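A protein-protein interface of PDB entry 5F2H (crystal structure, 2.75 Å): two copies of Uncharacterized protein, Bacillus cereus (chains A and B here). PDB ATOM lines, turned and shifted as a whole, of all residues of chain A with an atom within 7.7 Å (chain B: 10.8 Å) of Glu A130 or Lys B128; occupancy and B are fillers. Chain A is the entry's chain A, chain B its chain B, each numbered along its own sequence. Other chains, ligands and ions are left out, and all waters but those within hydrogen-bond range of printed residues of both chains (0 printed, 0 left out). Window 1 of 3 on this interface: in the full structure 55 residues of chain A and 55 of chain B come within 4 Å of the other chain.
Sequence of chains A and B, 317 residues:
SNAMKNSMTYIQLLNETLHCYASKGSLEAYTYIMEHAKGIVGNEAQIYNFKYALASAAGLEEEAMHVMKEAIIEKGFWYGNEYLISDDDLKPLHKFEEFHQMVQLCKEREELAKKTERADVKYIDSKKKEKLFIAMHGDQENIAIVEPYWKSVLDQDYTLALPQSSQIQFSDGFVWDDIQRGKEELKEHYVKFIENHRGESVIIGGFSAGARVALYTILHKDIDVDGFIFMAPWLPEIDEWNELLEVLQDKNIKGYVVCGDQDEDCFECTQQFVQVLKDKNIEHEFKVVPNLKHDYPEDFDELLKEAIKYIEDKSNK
Of the printed residues of chain B, Lys A129 touches Asp B157 (2.9 Å).
Of chain B, only Lys B128 (3.98 Å) comes within 4 Å of Glu A130.
Of the printed residues of chain B, Asp A157 touches Ser B126 and Lys B129.
Of the printed residues of chain B, Tyr A158 touches Ser B126.
No residue of chain B comes within 4 Å of His A197.
No residue of chain B comes within 4 Å of Arg A198.
No residue of chain B comes within 4 Å of Gly A199.
Val A202 touches none of the printed residues of chain B.
Of the printed residues of chain A, Ile B124 touches Leu A154 (3.2 Å) and Thr A159 (3.9 Å).
Printed residues of chain A within 4 Å of Asp B125: Thr A159 (3.6 Å).
Lys B128 touches just one residue of chain A: Glu A130.
Asn B196 touches none of the printed residues of chain A.
Lys A129 touches Asp B157, and with the chains exchanged Asp A157 touches Lys B129.
13 positions are printed for both chains.
NZ of Lys A129 lies within salt-bridge range of OD2 of Asp B157 (2.9 Å).
Hydrophobic or aromatic side chains of chain B within 4 Å of the printed part of chain A: Ile B124.
Of the 17 printed residues of chain A, 6 touch a printed residue of chain B.
Among the printed residues, 9 pairs touch across the chains.
The backbone carbonyl oxygen of His A197 lies close to the side-chain carboxylate of Glu A130, at 2.5 Å.
The backbone carbonyl oxygen of Glu A130 sits at hydrogen-bond distance from the backbone NH of Glu A200, 3.1 Å away.
The backbone carbonyl oxygen (O) of Lys A131 is in hydrogen-bond range of the backbone NH (N) of Thr A159, 2.9 Å away.
The side-chain hydroxyl (OH) of Tyr A158 sits at hydrogen-bond distance from the side-chain hydroxyl (OG) of Ser A201, at 3.1 Å.
Among the printed residues, merely in contact across the chains: Glu A130 with Lys B128 (3.98 Å), Leu A154 with Ile B124 (3.2 Å), Asp A157 with Ser B126 (3.9 Å), Asp A157 with Lys B129 (3.3 Å), Tyr A158 with Ser B126 (3.9 Å), Thr A159 with Ile B124 (3.9 Å), Thr A159 with Asp B125 (3.6 Å) and Thr A159 with Ser B126 (3.9 Å).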
ATOM      1  N   LYS A 129      -7.476 -17.078  30.395  1.00  0.00           N
ATOM      2  CA  LYS A 129      -7.848 -16.507  31.684  1.00  0.00           C
ATOM      3  C   LYS A 129      -8.142 -15.014  31.597  1.00  0.00           C
ATOM      4  O   LYS A 129      -9.255 -14.592  31.867  1.00  0.00           O
ATOM      5  CB  LYS A 129      -6.738 -16.722  32.708  1.00  0.00           C
ATOM      6  CG  LYS A 129      -6.348 -18.169  32.895  1.00  0.00           C
ATOM      7  CD  LYS A 129      -5.240 -18.292  33.923  1.00  0.00           C
ATOM      8  CE  LYS A 129      -4.749 -19.724  33.986  1.00  0.00           C
ATOM      9  NZ  LYS A 129      -3.672 -19.924  34.994  1.00  0.00           N
ATOM     10  N   GLU A 130      -7.125 -14.222  31.261  1.00  0.00           N
ATOM     11  CA  GLU A 130      -7.238 -12.763  31.127  1.00  0.00           C
ATOM     12  C   GLU A 130      -7.415 -12.093  32.489  1.00  0.00           C
ATOM     13  O   GLU A 130      -8.530 -11.836  32.937  1.00  0.00           O
ATOM     14  CB  GLU A 130      -8.389 -12.409  30.179  1.00  0.00           C
ATOM     15  CG  GLU A 130      -8.245 -13.029  28.789  1.00  0.00           C
ATOM     16  CD  GLU A 130      -9.437 -12.775  27.882  1.00  0.00           C
ATOM     17  OE1 GLU A 130     -10.170 -11.803  28.131  1.00  0.00           O
ATOM     18  OE2 GLU A 130      -9.628 -13.534  26.901  1.00  0.00           O
ATOM     19  N   LYS A 131      -6.291 -11.781  33.124  1.00  0.00           N
ATOM     20  CA  LYS A 131      -6.277 -11.161  34.446  1.00  0.00           C
ATOM     21  C   LYS A 131      -5.904  -9.684  34.362  1.00  0.00           C
ATOM     22  O   LYS A 131      -5.117  -9.288  33.515  1.00  0.00           O
ATOM     23  CB  LYS A 131      -5.274 -11.910  35.331  1.00  0.00           C
ATOM     24  CG  LYS A 131      -5.578 -13.387  35.451  1.00  0.00           C
ATOM     25  CD  LYS A 131      -4.591 -14.073  36.365  1.00  0.00           C
ATOM     26  CE  LYS A 131      -5.051 -15.495  36.616  1.00  0.00           C
ATOM     27  NZ  LYS A 131      -4.114 -16.263  37.479  1.00  0.00           N
ATOM     28  N   LEU A 132      -6.443  -8.871  35.259  1.00  0.00           N
ATOM     29  CA  LEU A 132      -6.139  -7.441  35.250  1.00  0.00           C
ATOM     30  C   LEU A 132      -5.614  -6.943  36.572  1.00  0.00           C
ATOM     31  O   LEU A 132      -6.053  -7.395  37.630  1.00  0.00           O
ATOM     32  CB  LEU A 132      -7.392  -6.636  34.919  1.00  0.00           C
ATOM     33  CG  LEU A 132      -7.255  -5.111  34.952  1.00  0.00           C
ATOM     34  CD1 LEU A 132      -6.170  -4.583  34.030  1.00  0.00           C
ATOM     35  CD2 LEU A 132      -8.571  -4.478  34.567  1.00  0.00           C
ATOM     36  N   LEU A 154       3.407  -8.800  35.637  1.00  0.00           N
ATOM     37  CA  LEU A 154       3.298  -9.532  34.378  1.00  0.00           C
ATOM     38  C   LEU A 154       3.773 -10.966  34.601  1.00  0.00           C
ATOM     39  O   LEU A 154       3.291 -11.897  33.958  1.00  0.00           O
ATOM     40  CB  LEU A 154       4.130  -8.859  33.292  1.00  0.00           C
ATOM     41  CG  LEU A 154       3.823  -7.386  32.995  1.00  0.00           C
ATOM     42  CD1 LEU A 154       4.777  -6.882  31.921  1.00  0.00           C
ATOM     43  CD2 LEU A 154       2.376  -7.177  32.574  1.00  0.00           C
ATOM     44  N   ASP A 157       1.043 -13.367  35.186  1.00  0.00           N
ATOM     45  CA  ASP A 157       0.083 -13.377  34.094  1.00  0.00           C
ATOM     46  C   ASP A 157      -0.972 -12.282  34.173  1.00  0.00           C
ATOM     47  O   ASP A 157      -2.093 -12.481  33.723  1.00  0.00           O
ATOM     48  CB  ASP A 157      -0.573 -14.762  33.999  1.00  0.00           C
ATOM     49  CG  ASP A 157       0.445 -15.874  33.777  1.00  0.00           C
ATOM     50  OD1 ASP A 157       1.632 -15.551  33.531  1.00  0.00           O
ATOM     51  OD2 ASP A 157       0.057 -17.066  33.824  1.00  0.00           O
ATOM     52  N   TYR A 158      -0.614 -11.123  34.728  1.00  0.00           N
ATOM     53  CA  TYR A 158      -1.552  -9.993  34.842  1.00  0.00           C
ATOM     54  C   TYR A 158      -1.299  -8.850  33.886  1.00  0.00           C
ATOM     55  O   TYR A 158      -0.177  -8.361  33.777  1.00  0.00           O
ATOM     56  CB  TYR A 158      -1.535  -9.367  36.244  1.00  0.00           C
ATOM     57  CG  TYR A 158      -2.313 -10.100  37.300  1.00  0.00           C
ATOM     58  CD1 TYR A 158      -1.736 -11.120  38.036  1.00  0.00           C
ATOM     59  CD2 TYR A 158      -3.617  -9.721  37.599  1.00  0.00           C
ATOM     60  CE1 TYR A 158      -2.452 -11.772  39.020  1.00  0.00           C
ATOM     61  CE2 TYR A 158      -4.342 -10.370  38.575  1.00  0.00           C
ATOM     62  CZ  TYR A 158      -3.755 -11.394  39.285  1.00  0.00           C
ATOM     63  OH  TYR A 158      -4.473 -12.056  40.257  1.00  0.00           O
ATOM     64  N   THR A 159      -2.362  -8.405  33.227  1.00  0.00           N
ATOM     65  CA  THR A 159      -2.289  -7.273  32.316  1.00  0.00           C
ATOM     66  C   THR A 159      -2.233  -6.070  33.247  1.00  0.00           C
ATOM     67  O   THR A 159      -3.061  -5.967  34.135  1.00  0.00           O
ATOM     68  CB  THR A 159      -3.534  -7.200  31.413  1.00  0.00           C
ATOM     69  OG1 THR A 159      -3.583  -8.364  30.571  1.00  0.00           O
ATOM     70  CG2 THR A 159      -3.514  -5.947  30.551  1.00  0.00           C
ATOM     71  N   PHE A 193     -12.349  -1.521  29.890  1.00  0.00           N
ATOM     72  CA  PHE A 193     -11.583  -2.749  29.830  1.00  0.00           C
ATOM     73  C   PHE A 193     -12.423  -4.020  29.869  1.00  0.00           C
ATOM     74  O   PHE A 193     -12.186  -4.930  29.089  1.00  0.00           O
ATOM     75  CB  PHE A 193     -10.603  -2.805  30.972  1.00  0.00           C
ATOM     76  CG  PHE A 193      -9.784  -4.044  30.970  1.00  0.00           C
ATOM     77  CD1 PHE A 193     -10.261  -5.210  31.554  1.00  0.00           C
ATOM     78  CD2 PHE A 193      -8.540  -4.057  30.362  1.00  0.00           C
ATOM     79  CE1 PHE A 193      -9.500  -6.364  31.544  1.00  0.00           C
ATOM     80  CE2 PHE A 193      -7.774  -5.202  30.357  1.00  0.00           C
ATOM     81  CZ  PHE A 193      -8.251  -6.358  30.948  1.00  0.00           C
ATOM     82  N   ILE A 194     -13.371  -4.117  30.796  1.00  0.00           N
ATOM     83  CA  ILE A 194     -14.203  -5.329  30.873  1.00  0.00           C
ATOM     84  C   ILE A 194     -15.203  -5.479  29.738  1.00  0.00           C
ATOM     85  O   ILE A 194     -15.542  -6.605  29.373  1.00  0.00           O
ATOM     86  CB  ILE A 194     -14.969  -5.501  32.213  1.00  0.00           C
ATOM     87  CG1 ILE A 194     -16.026  -4.402  32.402  1.00  0.00           C
ATOM     88  CG2 ILE A 194     -13.991  -5.574  33.373  1.00  0.00           C
ATOM     89  CD1 ILE A 194     -16.870  -4.577  33.646  1.00  0.00           C
ATOM     90  N   ASN A 196     -14.739  -5.387  26.795  1.00  0.00           N
ATOM     91  CA  ASN A 196     -14.047  -6.178  25.758  1.00  0.00           C
ATOM     92  C   ASN A 196     -13.018  -7.184  26.324  1.00  0.00           C
ATOM     93  O   ASN A 196     -12.053  -7.516  25.634  1.00  0.00           O
ATOM     94  CB  ASN A 196     -13.346  -5.254  24.734  1.00  0.00           C
ATOM     95  CG  ASN A 196     -14.320  -4.447  23.885  1.00  0.00           C
ATOM     96  OD1 ASN A 196     -15.516  -4.736  23.823  1.00  0.00           O
ATOM     97  ND2 ASN A 196     -13.790  -3.461  23.172  1.00  0.00           N
ATOM     98  N   HIS A 197     -13.222  -7.686  27.549  1.00  0.00           N
ATOM     99  CA  HIS A 197     -12.278  -8.646  28.155  1.00  0.00           C
ATOM    100  C   HIS A 197     -12.763  -9.694  29.172  1.00  0.00           C
ATOM    101  O   HIS A 197     -12.039 -10.668  29.384  1.00  0.00           O
ATOM    102  CB  HIS A 197     -11.082  -7.909  28.747  1.00  0.00           C
ATOM    103  CG  HIS A 197     -10.204  -7.266  27.726  1.00  0.00           C
ATOM    104  ND1 HIS A 197     -10.450  -6.008  27.218  1.00  0.00           N
ATOM    105  CD2 HIS A 197      -9.063  -7.694  27.138  1.00  0.00           C
ATOM    106  CE1 HIS A 197      -9.508  -5.695  26.347  1.00  0.00           C
ATOM    107  NE2 HIS A 197      -8.652  -6.701  26.283  1.00  0.00           N
ATOM    108  N   ARG A 198     -13.890  -9.502  29.863  1.00  0.00           N
ATOM    109  CA  ARG A 198     -14.367 -10.547  30.799  1.00  0.00           C
ATOM    110  C   ARG A 198     -13.344 -10.907  31.882  1.00  0.00           C
ATOM    111  O   ARG A 198     -13.426 -11.970  32.509  1.00  0.00           O
ATOM    112  CB  ARG A 198     -14.786 -11.783  29.951  1.00  0.00           C
ATOM    113  CG  ARG A 198     -14.886 -13.170  30.594  1.00  0.00           C
ATOM    114  CD  ARG A 198     -15.528 -14.128  29.580  1.00  0.00           C
ATOM    115  NE  ARG A 198     -15.289 -15.559  29.799  1.00  0.00           N
ATOM    116  CZ  ARG A 198     -14.393 -16.286  29.122  1.00  0.00           C
ATOM    117  NH1 ARG A 198     -14.259 -17.576  29.387  1.00  0.00           N
ATOM    118  NH2 ARG A 198     -13.644 -15.745  28.164  1.00  0.00           N
ATOM    119  N   GLY A 199     -12.435  -9.968  32.142  1.00  0.00           N
ATOM    120  CA  GLY A 199     -11.369 -10.134  33.123  1.00  0.00           C
ATOM    121  C   GLY A 199     -11.804 -10.995  34.288  1.00  0.00           C
ATOM    122  O   GLY A 199     -12.651 -10.579  35.072  1.00  0.00           O
ATOM    123  N   GLU A 200     -11.239 -12.196  34.401  1.00  0.00           N
ATOM    124  CA  GLU A 200     -11.592 -13.072  35.506  1.00  0.00           C
ATOM    125  C   GLU A 200     -11.168 -12.642  36.898  1.00  0.00           C
ATOM    126  O   GLU A 200     -12.022 -12.265  37.702  1.00  0.00           O
ATOM    127  CB  GLU A 200     -11.014 -14.481  35.328  1.00  0.00           C
ATOM    128  CG  GLU A 200     -11.558 -15.215  34.100  1.00  0.00           C
ATOM    129  CD  GLU A 200     -13.068 -15.457  34.118  1.00  0.00           C
ATOM    130  OE1 GLU A 200     -13.627 -15.774  33.042  1.00  0.00           O
ATOM    131  OE2 GLU A 200     -13.708 -15.322  35.185  1.00  0.00           O
ATOM    132  N   SER A 201      -9.868 -12.625  37.167  1.00  0.00           N
ATOM    133  CA  SER A 201      -9.334 -12.020  38.385  1.00  0.00           C
ATOM    134  C   SER A 201      -8.948 -10.550  38.206  1.00  0.00           C
ATOM    135  O   SER A 201      -8.420 -10.163  37.169  1.00  0.00           O
ATOM    136  CB  SER A 201      -8.120 -12.798  38.875  1.00  0.00           C
ATOM    137  OG  SER A 201      -7.581 -12.201  40.044  1.00  0.00           O
ATOM    138  N   VAL A 202      -9.234  -9.738  39.226  1.00  0.00           N
ATOM    139  CA  VAL A 202      -8.910  -8.308  39.213  1.00  0.00           C
ATOM    140  C   VAL A 202      -8.386  -7.842  40.582  1.00  0.00           C
ATOM    141  O   VAL A 202      -9.062  -7.983  41.598  1.00  0.00           O
ATOM    142  CB  VAL A 202     -10.120  -7.433  38.823  1.00  0.00           C
ATOM    143  CG1 VAL A 202      -9.718  -5.962  38.812  1.00  0.00           C
ATOM    144  CG2 VAL A 202     -10.634  -7.843  37.454  1.00  0.00           C
ATOM    145  N   ILE B 124      -0.107  -2.519  29.711  1.00  0.00           N
ATOM    146  CA  ILE B 124       1.085  -3.316  29.440  1.00  0.00           C
ATOM    147  C   ILE B 124       0.629  -4.769  29.516  1.00  0.00           C
ATOM    148  O   ILE B 124       0.668  -5.397  30.578  1.00  0.00           O
ATOM    149  CB  ILE B 124       2.186  -3.050  30.478  1.00  0.00           C
ATOM    150  CG1 ILE B 124       2.553  -1.575  30.499  1.00  0.00           C
ATOM    151  CG2 ILE B 124       3.421  -3.875  30.188  1.00  0.00           C
ATOM    152  CD1 ILE B 124       3.667  -1.249  31.471  1.00  0.00           C
ATOM    153  N   ASP B 125       0.153  -5.279  28.386  1.00  0.00           N
ATOM    154  CA  ASP B 125      -0.349  -6.653  28.289  1.00  0.00           C
ATOM    155  C   ASP B 125       0.693  -7.712  28.664  1.00  0.00           C
ATOM    156  O   ASP B 125       1.897  -7.527  28.467  1.00  0.00           O
ATOM    157  CB  ASP B 125      -0.859  -6.929  26.874  1.00  0.00           C
ATOM    158  CG  ASP B 125      -1.951  -5.958  26.440  1.00  0.00           C
ATOM    159  OD1 ASP B 125      -2.350  -5.090  27.242  1.00  0.00           O
ATOM    160  OD2 ASP B 125      -2.408  -6.056  25.284  1.00  0.00           O
ATOM    161  N   SER B 126       0.200  -8.819  29.214  1.00  0.00           N
ATOM    162  CA  SER B 126       1.041  -9.932  29.628  1.00  0.00           C
ATOM    163  C   SER B 126       1.402 -10.779  28.408  1.00  0.00           C
ATOM    164  O   SER B 126       0.807 -10.625  27.341  1.00  0.00           O
ATOM    165  CB  SER B 126       0.322 -10.760  30.688  1.00  0.00           C
ATOM    166  OG  SER B 126      -0.921 -11.218  30.198  1.00  0.00           O
ATOM    167  N   LYS B 127       2.330 -11.713  28.580  1.00  0.00           N
ATOM    168  CA  LYS B 127       2.785 -12.544  27.466  1.00  0.00           C
ATOM    169  C   LYS B 127       1.991 -13.838  27.282  1.00  0.00           C
ATOM    170  O   LYS B 127       2.078 -14.478  26.235  1.00  0.00           O
ATOM    171  CB  LYS B 127       4.266 -12.900  27.676  1.00  0.00           C
ATOM    172  CG  LYS B 127       5.146 -11.734  28.131  1.00  0.00           C
ATOM    173  CD  LYS B 127       5.023 -10.485  27.265  1.00  0.00           C
ATOM    174  CE  LYS B 127       5.857  -9.339  27.832  1.00  0.00           C
ATOM    175  NZ  LYS B 127       5.689  -8.056  27.090  1.00  0.00           N
ATOM    176  N   LYS B 128       1.206 -14.203  28.288  1.00  0.00           N
ATOM    177  CA  LYS B 128       0.418 -15.435  28.274  1.00  0.00           C
ATOM    178  C   LYS B 128       1.294 -16.684  28.242  1.00  0.00           C
ATOM    179  O   LYS B 128       1.664 -17.205  27.182  1.00  0.00           O
ATOM    180  CB  LYS B 128      -0.669 -15.454  27.193  1.00  0.00           C
ATOM    181  CG  LYS B 128      -1.793 -14.481  27.504  1.00  0.00           C
ATOM    182  CD  LYS B 128      -2.987 -14.613  26.574  1.00  0.00           C
ATOM    183  CE  LYS B 128      -4.110 -13.683  27.027  1.00  0.00           C
ATOM    184  NZ  LYS B 128      -5.336 -13.801  26.190  1.00  0.00           N
ATOM    185  N   LYS B 129       1.617 -17.145  29.447  1.00  0.00           N
ATOM    186  CA  LYS B 129       2.439 -18.333  29.646  1.00  0.00           C
ATOM    187  C   LYS B 129       1.693 -19.587  29.191  1.00  0.00           C
ATOM    188  O   LYS B 129       1.074 -20.277  29.992  1.00  0.00           O
ATOM    189  CB  LYS B 129       2.821 -18.476  31.125  1.00  0.00           C
ATOM    190  CG  LYS B 129       3.716 -17.378  31.687  1.00  0.00           C
ATOM    191  CD  LYS B 129       4.154 -17.698  33.117  1.00  0.00           C
ATOM    192  CE  LYS B 129       5.043 -18.942  33.186  1.00  0.00           C
ATOM    193  NZ  LYS B 129       5.429 -19.316  34.575  1.00  0.00           N
ATOM    194  N   GLU B 130       1.761 -19.865  27.898  1.00  0.00           N
ATOM    195  CA  GLU B 130       1.099 -21.033  27.301  1.00  0.00           C
ATOM    196  C   GLU B 130       1.862 -22.346  27.582  1.00  0.00           C
ATOM    197  O   GLU B 130       3.028 -22.491  27.199  1.00  0.00           O
ATOM    198  CB  GLU B 130       0.958 -20.808  25.790  1.00  0.00           C
ATOM    199  CG  GLU B 130       2.306 -20.580  25.112  1.00  0.00           C
ATOM    200  CD  GLU B 130       2.219 -20.184  23.656  1.00  0.00           C
ATOM    201  OE1 GLU B 130       3.257 -20.275  22.949  1.00  0.00           O
ATOM    202  OE2 GLU B 130       1.126 -19.767  23.223  1.00  0.00           O
ATOM    203  N   LYS B 131       1.203 -23.294  28.249  1.00  0.00           N
ATOM    204  CA  LYS B 131       1.807 -24.591  28.587  1.00  0.00           C
ATOM    205  C   LYS B 131       1.256 -25.663  27.641  1.00  0.00           C
ATOM    206  O   LYS B 131       0.099 -25.589  27.229  1.00  0.00           O
ATOM    207  CB  LYS B 131       1.510 -24.941  30.053  1.00  0.00           C
ATOM    208  CG  LYS B 131       2.005 -23.865  31.020  1.00  0.00           C
ATOM    209  CD  LYS B 131       1.686 -24.062  32.505  1.00  0.00           C
ATOM    210  CE  LYS B 131       2.404 -25.250  33.121  1.00  0.00           C
ATOM    211  NZ  LYS B 131       2.141 -25.394  34.584  1.00  0.00           N
ATOM    212  N   LEU B 132       2.076 -26.652  27.286  1.00  0.00           N
ATOM    213  CA  LEU B 132       1.630 -27.703  26.374  1.00  0.00           C
ATOM    214  C   LEU B 132       1.794 -29.072  26.954  1.00  0.00           C
ATOM    215  O   LEU B 132       2.733 -29.329  27.679  1.00  0.00           O
ATOM    216  CB  LEU B 132       2.408 -27.650  25.055  1.00  0.00           C
ATOM    217  CG  LEU B 132       2.103 -28.755  24.033  1.00  0.00           C
ATOM    218  CD1 LEU B 132       0.633 -28.818  23.649  1.00  0.00           C
ATOM    219  CD2 LEU B 132       2.926 -28.544  22.778  1.00  0.00           C
ATOM    220  N   ASP B 157      -3.719 -25.724  33.771  1.00  0.00           N
ATOM    221  CA  ASP B 157      -3.465 -24.700  32.771  1.00  0.00           C
ATOM    222  C   ASP B 157      -2.689 -25.197  31.557  1.00  0.00           C
ATOM    223  O   ASP B 157      -1.929 -24.437  30.972  1.00  0.00           O
ATOM    224  CB  ASP B 157      -2.699 -23.539  33.427  1.00  0.00           C
ATOM    225  CG  ASP B 157      -2.719 -22.263  32.596  1.00  0.00           C
ATOM    226  OD1 ASP B 157      -3.384 -22.235  31.538  1.00  0.00           O
ATOM    227  OD2 ASP B 157      -2.086 -21.269  33.023  1.00  0.00           O
ATOM    228  N   THR B 159      -2.528 -26.767  27.648  1.00  0.00           N
ATOM    229  CA  THR B 159      -3.205 -26.947  26.366  1.00  0.00           C
ATOM    230  C   THR B 159      -2.928 -28.400  26.028  1.00  0.00           C
ATOM    231  O   THR B 159      -1.779 -28.837  26.076  1.00  0.00           O
ATOM    232  CB  THR B 159      -2.606 -26.030  25.290  1.00  0.00           C
ATOM    233  OG1 THR B 159      -2.834 -24.663  25.659  1.00  0.00           O
ATOM    234  CG2 THR B 159      -3.222 -26.311  23.922  1.00  0.00           C
ATOM    235  N   PHE B 193       3.415 -26.369  16.344  1.00  0.00           N
ATOM    236  CA  PHE B 193       2.904 -25.725  17.539  1.00  0.00           C
ATOM    237  C   PHE B 193       3.803 -24.629  18.072  1.00  0.00           C
ATOM    238  O   PHE B 193       3.321 -23.555  18.390  1.00  0.00           O
ATOM    239  CB  PHE B 193       2.660 -26.729  18.662  1.00  0.00           C
ATOM    240  CG  PHE B 193       2.114 -26.099  19.925  1.00  0.00           C
ATOM    241  CD1 PHE B 193       2.972 -25.554  20.868  1.00  0.00           C
ATOM    242  CD2 PHE B 193       0.744 -26.054  20.170  1.00  0.00           C
ATOM    243  CE1 PHE B 193       2.475 -24.979  22.031  1.00  0.00           C
ATOM    244  CE2 PHE B 193       0.244 -25.490  21.336  1.00  0.00           C
ATOM    245  CZ  PHE B 193       1.112 -24.948  22.265  1.00  0.00           C
ATOM    246  N   ASN B 196       4.262 -21.070  15.804  1.00  0.00           N
ATOM    247  CA  ASN B 196       3.235 -20.045  15.910  1.00  0.00           C
ATOM    248  C   ASN B 196       2.846 -19.794  17.369  1.00  0.00           C
ATOM    249  O   ASN B 196       1.712 -19.423  17.664  1.00  0.00           O
ATOM    250  CB  ASN B 196       2.023 -20.531  15.115  1.00  0.00           C
ATOM    251  CG  ASN B 196       0.990 -19.452  14.883  1.00  0.00           C
ATOM    252  OD1 ASN B 196       1.116 -18.329  15.366  1.00  0.00           O
ATOM    253  ND2 ASN B 196      -0.032 -19.786  14.108  1.00  0.00           N
ATOM    254  N   HIS B 197       3.781 -20.026  18.285  1.00  0.00           N
ATOM    255  CA  HIS B 197       3.524 -19.824  19.706  1.00  0.00           C
ATOM    256  C   HIS B 197       4.808 -19.603  20.502  1.00  0.00           C
ATOM    257  O   HIS B 197       5.122 -18.493  20.919  1.00  0.00           O
ATOM    258  CB  HIS B 197       2.800 -21.038  20.303  1.00  0.00           C
ATOM    259  CG  HIS B 197       1.410 -21.241  19.795  1.00  0.00           C
ATOM    260  ND1 HIS B 197       1.135 -21.930  18.634  1.00  0.00           N
ATOM    261  CD2 HIS B 197       0.212 -20.894  20.320  1.00  0.00           C
ATOM    262  CE1 HIS B 197      -0.173 -21.967  18.448  1.00  0.00           C
ATOM    263  NE2 HIS B 197      -0.756 -21.350  19.460  1.00  0.00           N
ATOM    264  N   ARG B 198       5.546 -20.694  20.670  1.00  0.00           N
ATOM    265  CA  ARG B 198       6.792 -20.757  21.435  1.00  0.00           C
ATOM    266  C   ARG B 198       6.472 -20.684  22.927  1.00  0.00           C
ATOM    267  O   ARG B 198       6.720 -19.683  23.599  1.00  0.00           O
ATOM    268  CB  ARG B 198       7.839 -19.721  21.022  1.00  0.00           C
ATOM    269  CG  ARG B 198       9.183 -19.921  21.724  1.00  0.00           C
ATOM    270  CD  ARG B 198       9.791 -21.269  21.339  1.00  0.00           C
ATOM    271  NE  ARG B 198      11.022 -21.605  22.060  1.00  0.00           N
ATOM    272  CZ  ARG B 198      11.075 -22.290  23.206  1.00  0.00           C
ATOM    273  NH1 ARG B 198       9.967 -22.715  23.807  1.00  0.00           N
ATOM    274  NH2 ARG B 198      12.251 -22.542  23.769  1.00  0.00           N
ATOM    275  N   GLY B 199       5.877 -21.766  23.412  1.00  0.00           N
ATOM    276  CA  GLY B 199       5.492 -21.897  24.810  1.00  0.00           C
ATOM    277  C   GLY B 199       6.617 -22.167  25.789  1.00  0.00           C
ATOM    278  O   GLY B 199       7.773 -22.392  25.405  1.00  0.00           O
ATOM    279  N   GLU B 200       6.244 -22.136  27.068  1.00  0.00           N
ATOM    280  CA  GLU B 200       7.157 -22.365  28.186  1.00  0.00           C
ATOM    281  C   GLU B 200       7.286 -23.848  28.557  1.00  0.00           C
ATOM    282  O   GLU B 200       8.116 -24.559  27.984  1.00  0.00           O
ATOM    283  CB  GLU B 200       6.753 -21.530  29.419  1.00  0.00           C
ATOM    284  CG  GLU B 200       6.791 -20.009  29.263  1.00  0.00           C
ATOM    285  CD  GLU B 200       5.735 -19.428  28.329  1.00  0.00           C
ATOM    286  OE1 GLU B 200       4.787 -20.143  27.952  1.00  0.00           O
ATOM    287  OE2 GLU B 200       5.823 -18.224  28.007  1.00  0.00           O
ATOM    288  N   SER B 201       6.458 -24.331  29.481  1.00  0.00           N
ATOM    289  CA  SER B 201       6.537 -25.723  29.917  1.00  0.00           C
ATOM    290  C   SER B 201       5.924 -26.718  28.939  1.00  0.00           C
ATOM    291  O   SER B 201       4.885 -26.441  28.342  1.00  0.00           O
ATOM    292  CB  SER B 201       5.860 -25.881  31.284  1.00  0.00           C
ATOM    293  OG  SER B 201       5.905 -27.232  31.730  1.00  0.00           O
